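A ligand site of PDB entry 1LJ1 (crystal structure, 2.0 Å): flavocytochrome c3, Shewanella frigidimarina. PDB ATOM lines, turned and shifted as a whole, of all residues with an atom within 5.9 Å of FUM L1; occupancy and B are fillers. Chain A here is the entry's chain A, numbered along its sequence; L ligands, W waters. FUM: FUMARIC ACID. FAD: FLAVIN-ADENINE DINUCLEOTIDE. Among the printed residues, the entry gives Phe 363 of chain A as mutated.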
ATOM      1  N   ALA A 168      31.061 -28.562  18.014  1.00  0.00           N
ATOM      2  CA  ALA A 168      30.476 -27.257  18.380  1.00  0.00           C
ATOM      3  C   ALA A 168      30.020 -26.441  17.191  1.00  0.00           C
ATOM      4  O   ALA A 168      30.665 -26.439  16.126  1.00  0.00           O
ATOM      5  CB  ALA A 168      31.405 -26.419  19.248  1.00  0.00           C
ATOM      6  N   ALA A 169      28.939 -25.644  17.443  1.00  0.00           N
ATOM      7  CA  ALA A 169      28.360 -24.864  16.371  1.00  0.00           C
ATOM      8  C   ALA A 169      28.237 -23.374  16.600  1.00  0.00           C
ATOM      9  O   ALA A 169      28.974 -22.545  15.960  1.00  0.00           O
ATOM     10  CB  ALA A 169      26.985 -25.522  16.035  1.00  0.00           C
ATOM     11  N   GLY A 170      27.362 -22.932  17.483  1.00  0.00           N
ATOM     12  CA  GLY A 170      27.001 -21.563  17.707  1.00  0.00           C
ATOM     13  C   GLY A 170      28.086 -20.565  18.110  1.00  0.00           C
ATOM     14  O   GLY A 170      27.953 -19.396  17.701  1.00  0.00           O
ATOM     15  N   GLY A 171      29.110 -20.952  18.862  1.00  0.00           N
ATOM     16  CA  GLY A 171      30.156 -20.004  19.176  1.00  0.00           C
ATOM     17  C   GLY A 171      30.903 -20.102  20.481  1.00  0.00           C
ATOM     18  O   GLY A 171      30.659 -20.899  21.381  1.00  0.00           O
ATOM     19  N   MET A 236      23.192 -15.570  21.530  1.00  0.00           N
ATOM     20  CA  MET A 236      22.803 -16.899  22.013  1.00  0.00           C
ATOM     21  C   MET A 236      21.841 -16.695  23.185  1.00  0.00           C
ATOM     22  O   MET A 236      21.754 -15.554  23.620  1.00  0.00           O
ATOM     23  CB  MET A 236      23.967 -17.776  22.453  1.00  0.00           C
ATOM     24  CG  MET A 236      24.910 -18.112  21.300  1.00  0.00           C
ATOM     25  SD  MET A 236      24.244 -19.332  20.138  1.00  0.00           S
ATOM     26  CE  MET A 236      24.834 -20.819  20.951  1.00  0.00           C
ATOM     27  N   PHE A 363      22.386 -30.334  31.428  1.00  0.00           N
ATOM     28  CA  PHE A 363      21.855 -29.530  30.348  1.00  0.00           C
ATOM     29  C   PHE A 363      21.092 -30.402  29.342  1.00  0.00           C
ATOM     30  O   PHE A 363      21.605 -31.307  28.671  1.00  0.00           O
ATOM     31  CB  PHE A 363      23.027 -28.783  29.739  1.00  0.00           C
ATOM     32  CG  PHE A 363      22.873 -27.809  28.623  1.00  0.00           C
ATOM     33  CD1 PHE A 363      23.710 -26.713  28.586  1.00  0.00           C
ATOM     34  CD2 PHE A 363      21.997 -27.944  27.595  1.00  0.00           C
ATOM     35  CE1 PHE A 363      23.643 -25.783  27.565  1.00  0.00           C
ATOM     36  CE2 PHE A 363      21.884 -27.015  26.571  1.00  0.00           C
ATOM     37  CZ  PHE A 363      22.727 -25.921  26.550  1.00  0.00           C
ATOM     38  N   HIS A 365      19.450 -29.932  25.871  1.00  0.00           N
ATOM     39  CA  HIS A 365      19.362 -28.949  24.776  1.00  0.00           C
ATOM     40  C   HIS A 365      17.972 -29.098  24.181  1.00  0.00           C
ATOM     41  O   HIS A 365      17.531 -30.207  23.828  1.00  0.00           O
ATOM     42  CB  HIS A 365      20.443 -29.264  23.756  1.00  0.00           C
ATOM     43  CG  HIS A 365      20.671 -28.259  22.674  1.00  0.00           C
ATOM     44  ND1 HIS A 365      19.734 -27.896  21.725  1.00  0.00           N
ATOM     45  CD2 HIS A 365      21.798 -27.590  22.341  1.00  0.00           C
ATOM     46  CE1 HIS A 365      20.255 -27.000  20.895  1.00  0.00           C
ATOM     47  NE2 HIS A 365      21.513 -26.771  21.266  1.00  0.00           N
ATOM     48  N   THR A 367      16.731 -28.236  21.236  1.00  0.00           N
ATOM     49  CA  THR A 367      16.498 -28.495  19.817  1.00  0.00           C
ATOM     50  C   THR A 367      17.375 -29.531  19.109  1.00  0.00           C
ATOM     51  O   THR A 367      18.188 -29.197  18.209  1.00  0.00           O
ATOM     52  CB  THR A 367      16.498 -27.165  19.012  1.00  0.00           C
ATOM     53  OG1 THR A 367      17.796 -26.551  18.960  1.00  0.00           O
ATOM     54  CG2 THR A 367      15.550 -26.098  19.557  1.00  0.00           C
ATOM     55  N   MET A 375      22.062 -32.482  17.104  1.00  0.00           N
ATOM     56  CA  MET A 375      21.775 -31.104  17.536  1.00  0.00           C
ATOM     57  C   MET A 375      21.533 -30.122  16.382  1.00  0.00           C
ATOM     58  O   MET A 375      22.279 -30.115  15.400  1.00  0.00           O
ATOM     59  CB  MET A 375      22.976 -30.522  18.301  1.00  0.00           C
ATOM     60  CG  MET A 375      22.691 -29.289  19.159  1.00  0.00           C
ATOM     61  SD  MET A 375      24.208 -28.464  19.719  1.00  0.00           S
ATOM     62  CE  MET A 375      24.787 -27.884  18.120  1.00  0.00           C
ATOM     63  N   VAL A 376      20.629 -29.169  16.596  1.00  0.00           N
ATOM     64  CA  VAL A 376      20.404 -28.084  15.679  1.00  0.00           C
ATOM     65  C   VAL A 376      20.808 -26.848  16.502  1.00  0.00           C
ATOM     66  O   VAL A 376      20.220 -26.640  17.586  1.00  0.00           O
ATOM     67  CB  VAL A 376      18.965 -27.953  15.169  1.00  0.00           C
ATOM     68  CG1 VAL A 376      18.788 -26.675  14.309  1.00  0.00           C
ATOM     69  CG2 VAL A 376      18.428 -29.161  14.405  1.00  0.00           C
ATOM     70  N   THR A 377      21.762 -26.049  16.038  1.00  0.00           N
ATOM     71  CA  THR A 377      22.279 -24.974  16.888  1.00  0.00           C
ATOM     72  C   THR A 377      21.238 -23.943  17.277  1.00  0.00           C
ATOM     73  O   THR A 377      20.290 -23.508  16.608  1.00  0.00           O
ATOM     74  CB  THR A 377      23.522 -24.269  16.282  1.00  0.00           C
ATOM     75  OG1 THR A 377      23.990 -23.233  17.158  1.00  0.00           O
ATOM     76  CG2 THR A 377      23.262 -23.549  14.958  1.00  0.00           C
ATOM     77  N   GLU A 378      21.417 -23.468  18.496  1.00  0.00           N
ATOM     78  CA  GLU A 378      20.754 -22.357  19.145  1.00  0.00           C
ATOM     79  C   GLU A 378      21.021 -21.076  18.369  1.00  0.00           C
ATOM     80  O   GLU A 378      20.148 -20.172  18.415  1.00  0.00           O
ATOM     81  CB  GLU A 378      21.287 -22.187  20.572  1.00  0.00           C
ATOM     82  CG  GLU A 378      20.729 -21.060  21.413  1.00  0.00           C
ATOM     83  CD  GLU A 378      21.365 -20.982  22.785  1.00  0.00           C
ATOM     84  OE1 GLU A 378      22.492 -21.509  23.019  1.00  0.00           O
ATOM     85  OE2 GLU A 378      20.787 -20.370  23.664  1.00  0.00           O
ATOM     86  N   ALA A 379      22.108 -20.984  17.586  1.00  0.00           N
ATOM     87  CA  ALA A 379      22.349 -19.836  16.740  1.00  0.00           C
ATOM     88  C   ALA A 379      21.290 -19.668  15.642  1.00  0.00           C
ATOM     89  O   ALA A 379      21.128 -18.598  15.075  1.00  0.00           O
ATOM     90  CB  ALA A 379      23.743 -19.898  16.103  1.00  0.00           C
ATOM     91  N   ARG A 381      18.128 -19.802  16.252  1.00  0.00           N
ATOM     92  CA  ARG A 381      17.161 -18.913  16.921  1.00  0.00           C
ATOM     93  C   ARG A 381      17.826 -17.572  17.196  1.00  0.00           C
ATOM     94  O   ARG A 381      17.197 -16.535  16.996  1.00  0.00           O
ATOM     95  CB  ARG A 381      16.650 -19.563  18.210  1.00  0.00           C
ATOM     96  CG  ARG A 381      15.807 -20.811  18.051  1.00  0.00           C
ATOM     97  CD  ARG A 381      15.504 -21.494  19.396  1.00  0.00           C
ATOM     98  NE  ARG A 381      16.530 -22.501  19.724  1.00  0.00           N
ATOM     99  CZ  ARG A 381      17.100 -22.637  20.957  1.00  0.00           C
ATOM    100  NH1 ARG A 381      16.820 -21.843  21.992  1.00  0.00           N
ATOM    101  NH2 ARG A 381      17.980 -23.604  21.190  1.00  0.00           N
ATOM    102  N   HIS A 504      22.757 -33.149  26.611  1.00  0.00           N
ATOM    103  CA  HIS A 504      23.880 -32.480  25.901  1.00  0.00           C
ATOM    104  C   HIS A 504      25.129 -32.189  26.672  1.00  0.00           C
ATOM    105  O   HIS A 504      26.243 -32.157  26.114  1.00  0.00           O
ATOM    106  CB  HIS A 504      23.280 -31.125  25.391  1.00  0.00           C
ATOM    107  CG  HIS A 504      24.107 -30.196  24.548  1.00  0.00           C
ATOM    108  ND1 HIS A 504      24.609 -30.530  23.304  1.00  0.00           N
ATOM    109  CD2 HIS A 504      24.514 -28.899  24.777  1.00  0.00           C
ATOM    110  CE1 HIS A 504      25.259 -29.502  22.791  1.00  0.00           C
ATOM    111  NE2 HIS A 504      25.259 -28.498  23.686  1.00  0.00           N
ATOM    112  N   ARG A 544      24.143 -23.799  32.093  1.00  0.00           N
ATOM    113  CA  ARG A 544      25.213 -23.155  31.331  1.00  0.00           C
ATOM    114  C   ARG A 544      24.695 -22.273  30.217  1.00  0.00           C
ATOM    115  O   ARG A 544      23.696 -22.726  29.647  1.00  0.00           O
ATOM    116  CB  ARG A 544      26.103 -24.240  30.694  1.00  0.00           C
ATOM    117  CG  ARG A 544      27.306 -23.628  29.940  1.00  0.00           C
ATOM    118  CD  ARG A 544      28.199 -24.731  29.514  1.00  0.00           C
ATOM    119  NE  ARG A 544      27.743 -25.757  28.544  1.00  0.00           N
ATOM    120  CZ  ARG A 544      27.420 -25.521  27.293  1.00  0.00           C
ATOM    121  NH1 ARG A 544      27.114 -26.543  26.506  1.00  0.00           N
ATOM    122  NH2 ARG A 544      27.423 -24.266  26.798  1.00  0.00           N
ATOM    123  N   LEU A 545      25.329 -21.136  29.910  1.00  0.00           N
ATOM    124  CA  LEU A 545      24.825 -20.348  28.795  1.00  0.00           C
ATOM    125  C   LEU A 545      25.383 -20.910  27.481  1.00  0.00           C
ATOM    126  O   LEU A 545      26.525 -21.362  27.528  1.00  0.00           O
ATOM    127  CB  LEU A 545      25.237 -18.887  28.922  1.00  0.00           C
ATOM    128  CG  LEU A 545      24.700 -18.047  30.072  1.00  0.00           C
ATOM    129  CD1 LEU A 545      25.217 -16.614  29.941  1.00  0.00           C
ATOM    130  CD2 LEU A 545      23.166 -18.048  30.059  1.00  0.00           C
ATOM    131  N   GLY A 546      24.661 -20.832  26.385  1.00  0.00           N
ATOM    132  CA  GLY A 546      25.148 -21.242  25.078  1.00  0.00           C
ATOM    133  C   GLY A 546      26.391 -20.363  24.720  1.00  0.00           C
ATOM    134  O   GLY A 546      26.378 -19.156  24.917  1.00  0.00           O
ATOM    135  N   GLY A 547      27.466 -21.022  24.257  1.00  0.00           N
ATOM    136  CA  GLY A 547      28.723 -20.325  23.988  1.00  0.00           C
ATOM    137  C   GLY A 547      29.719 -20.342  25.138  1.00  0.00           C
ATOM    138  O   GLY A 547      30.935 -20.163  24.932  1.00  0.00           O
ATOM    139  N   ASN A 548      29.318 -20.615  26.377  1.00  0.00           N
ATOM    140  CA  ASN A 548      30.261 -20.563  27.473  1.00  0.00           C
ATOM    141  C   ASN A 548      31.148 -21.792  27.593  1.00  0.00           C
ATOM    142  O   ASN A 548      32.160 -21.689  28.298  1.00  0.00           O
ATOM    143  CB  ASN A 548      29.535 -20.257  28.801  1.00  0.00           C
ATOM    144  CG  ASN A 548      29.549 -18.757  29.113  1.00  0.00           C
ATOM    145  OD1 ASN A 548      30.097 -17.939  28.371  1.00  0.00           O
ATOM    146  ND2 ASN A 548      28.963 -18.382  30.248  1.00  0.00           N
ATOM    147  N   ALA A 549      30.809 -22.965  27.011  1.00  0.00           N
ATOM    148  CA  ALA A 549      31.701 -24.122  27.185  1.00  0.00           C
ATOM    149  C   ALA A 549      32.944 -24.065  26.299  1.00  0.00           C
ATOM    150  O   ALA A 549      34.044 -24.399  26.750  1.00  0.00           O
ATOM    151  CB  ALA A 549      30.918 -25.427  26.971  1.00  0.00           C
HETATM  152  OXT FUM L   1      25.131 -24.270  19.246  1.00  0.00           O
HETATM  153  C   FUM L   1      24.487 -24.753  20.192  1.00  0.00           C
HETATM  154  O   FUM L   1      23.182 -25.038  20.168  1.00  0.00           O
HETATM  155  C4  FUM L   1      25.103 -25.184  21.468  1.00  0.00           C
HETATM  156  C5  FUM L   1      25.684 -24.218  22.213  1.00  0.00           C
HETATM  157  C6  FUM L   1      26.288 -24.674  23.491  1.00  0.00           C
HETATM  158  O7  FUM L   1      26.975 -23.795  24.174  1.00  0.00           O
HETATM  159  O8  FUM L   1      26.158 -25.818  23.898  1.00  0.00           O
HETATM  160  PA  FAD L   2      35.725 -33.028  24.723  1.00  0.00           P
HETATM  161  O1A FAD L   2      34.558 -33.931  24.919  1.00  0.00           O
HETATM  162  O2A FAD L   2      35.839 -32.056  23.627  1.00  0.00           O
HETATM  163  O5B FAD L   2      37.041 -33.923  24.597  1.00  0.00           O
HETATM  164  C5B FAD L   2      37.452 -34.853  25.620  1.00  0.00           C
HETATM  165  C4B FAD L   2      38.168 -36.058  24.993  1.00  0.00           C
HETATM  166  O4B FAD L   2      38.636 -36.895  26.079  1.00  0.00           O
HETATM  167  C3B FAD L   2      37.305 -36.975  24.126  1.00  0.00           C
HETATM  168  O3B FAD L   2      37.913 -37.135  22.839  1.00  0.00           O
HETATM  169  C2B FAD L   2      37.266 -38.279  24.910  1.00  0.00           C
HETATM  170  O2B FAD L   2      37.181 -39.471  24.118  1.00  0.00           O
HETATM  171  C1B FAD L   2      38.676 -38.229  25.586  1.00  0.00           C
HETATM  172  N9A FAD L   2      38.644 -39.059  26.809  1.00  0.00           N
HETATM  173  C8A FAD L   2      37.644 -39.271  27.716  1.00  0.00           C
HETATM  174  N7A FAD L   2      38.009 -40.144  28.680  1.00  0.00           N
HETATM  175  C5A FAD L   2      39.321 -40.515  28.354  1.00  0.00           C
HETATM  176  C6A FAD L   2      40.269 -41.356  28.942  1.00  0.00           C
HETATM  177  N6A FAD L   2      40.093 -42.042  30.104  1.00  0.00           N
HETATM  178  N1A FAD L   2      41.490 -41.489  28.351  1.00  0.00           N
HETATM  179  C2A FAD L   2      41.748 -40.810  27.210  1.00  0.00           C
HETATM  180  N3A FAD L   2      40.882 -39.989  26.549  1.00  0.00           N
HETATM  181  C4A FAD L   2      39.701 -39.871  27.212  1.00  0.00           C
HETATM  182  N1  FAD L   2      29.675 -25.480  23.720  1.00  0.00           N
HETATM  183  C2  FAD L   2      29.717 -24.144  23.434  1.00  0.00           C
HETATM  184  O2  FAD L   2      30.038 -23.335  24.300  1.00  0.00           O
HETATM  185  N3  FAD L   2      29.393 -23.594  22.169  1.00  0.00           N
HETATM  186  C4  FAD L   2      28.996 -24.395  21.091  1.00  0.00           C
HETATM  187  O4  FAD L   2      28.720 -23.958  20.014  1.00  0.00           O
HETATM  188  C4X FAD L   2      28.754 -25.825  21.472  1.00  0.00           C
HETATM  189  N5  FAD L   2      28.170 -26.624  20.621  1.00  0.00           N
HETATM  190  C5X FAD L   2      28.136 -27.961  20.954  1.00  0.00           C
HETATM  191  C6  FAD L   2      27.679 -28.909  19.954  1.00  0.00           C
HETATM  192  C7  FAD L   2      27.601 -30.269  20.214  1.00  0.00           C
HETATM  193  C7M FAD L   2      27.021 -31.254  19.192  1.00  0.00           C
HETATM  194  C8  FAD L   2      28.102 -30.758  21.443  1.00  0.00           C
HETATM  195  C8M FAD L   2      28.024 -32.280  21.755  1.00  0.00           C
HETATM  196  C9  FAD L   2      28.584 -29.853  22.442  1.00  0.00           C
HETATM  197  C9A FAD L   2      28.585 -28.446  22.207  1.00  0.00           C
HETATM  198  N10 FAD L   2      28.993 -27.532  23.164  1.00  0.00           N
HETATM  199  C10 FAD L   2      29.163 -26.233  22.782  1.00  0.00           C
HETATM  200  C1' FAD L   2      29.743 -28.054  24.393  1.00  0.00           C
HETATM  201  C2' FAD L   2      31.201 -28.169  24.121  1.00  0.00           C
HETATM  202  O2' FAD L   2      31.574 -28.605  22.776  1.00  0.00           O
HETATM  203  C3' FAD L   2      31.770 -29.363  25.060  1.00  0.00           C
HETATM  204  O3' FAD L   2      31.434 -28.837  26.382  1.00  0.00           O
HETATM  205  C4' FAD L   2      33.309 -29.442  24.978  1.00  0.00           C
HETATM  206  O4' FAD L   2      33.421 -30.419  23.884  1.00  0.00           O
HETATM  207  C5' FAD L   2      34.061 -29.892  26.231  1.00  0.00           C
HETATM  208  O5' FAD L   2      35.356 -29.922  25.594  1.00  0.00           O
HETATM  209  P   FAD L   2      36.438 -30.772  26.431  1.00  0.00           P
HETATM  210  O1P FAD L   2      37.805 -30.564  25.871  1.00  0.00           O
HETATM  211  O2P FAD L   2      36.308 -30.533  27.878  1.00  0.00           O
HETATM  212  O3P FAD L   2      35.950 -32.257  26.113  1.00  0.00           O
HETATM  213  O   HOH W   1      22.509 -24.095  23.512  1.00  0.00           O
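The side-chain sulfur (SD) of Met 375 sits close to an oxygen (O) of FUM L1, 3.6 Å away.
Ala 169 touches FUM L1.
CE of Met 236 touches C5 of FUM L1 (3.7 Å).
Gly 546 touches FUM L1.
Hydrophobic or aromatic side chains that line FUM L1: Ala 169, Met 236, His 365, Met 375 and His 504.
Of the 21 residues printed, 11 come within 4 Å of FUM L1.
The nearest printed residue that does not touch FUM L1 is Leu 545 (4.2 Å).
An oxygen (O7) of FUM L1 sits close to a nitrogen (N3) of FAD L2, at 3.1 Å.
The backbone NH of Gly 170 lies within hydrogen-bond range of the side-chain hydroxyl of Thr 377, at 3.4 Å.
N of Ala 379 sits at hydrogen-bond distance from OG1 of Thr 377 (3.0 Å).
The side-chain sulfur (SD) of Met 375 sits close to a ring nitrogen (NE2) of His 365.
A ring nitrogen (ND1) of His 365 is in hydrogen-bond range of the backbone NH (N) of Thr 367 (3.1 Å).
The backbone carbonyl oxygen (O) of Phe 363 lies within hydrogen-bond range of the backbone NH (N) of His 504 (3.0 Å).
N of Ala 379 sits at hydrogen-bond distance from SD of Met 236 (3.7 Å).
An oxygen (OXT) of FUM L1 sits at hydrogen-bond distance from the side-chain hydroxyl of Thr 377 (2.6 Å).
NE2 of His 365 is in hydrogen-bond range of O of FUM L1 (2.6 Å).
The guanidinium group of Arg 544 lies within salt-bridge range of an oxygen (O7) of FUM L1 (2.7 Å).
O7 of FUM L1 lies within hydrogen-bond range of N of Gly 547, at 2.8 Å.
NE2 of His 504 is in hydrogen-bond range of O8 of FUM L1.
O of FUM L1 sits at hydrogen-bond distance from N of Glu 378.
The backbone NH of Gly 170 lies within hydrogen-bond range of an oxygen (OXT) of FUM L1.
An oxygen (O2) of FAD L2 lies close to the backbone NH (N) of Gly 547, at 3.5 Å.
The backbone NH (N) of Gly 170 sits at hydrogen-bond distance from an oxygen (O4) of FAD L2.
N of Ala 169 lies within hydrogen-bond range of O4 of FAD L2 (3.1 Å).
O2 of FAD L2 is in hydrogen-bond range of N of Asn 548, at 3.5 Å.
O2 of FAD L2 sits at hydrogen-bond distance from N of Ala 549 (2.8 Å).
The backbone NH (N) of Gly 171 is in hydrogen-bond range of an oxygen (O4) of FAD L2, at 3.2 Å.
The backbone carbonyl oxygen of Gly 171 lies within hydrogen-bond range of a nitrogen (N3) of FAD L2, at 3.1 Å.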
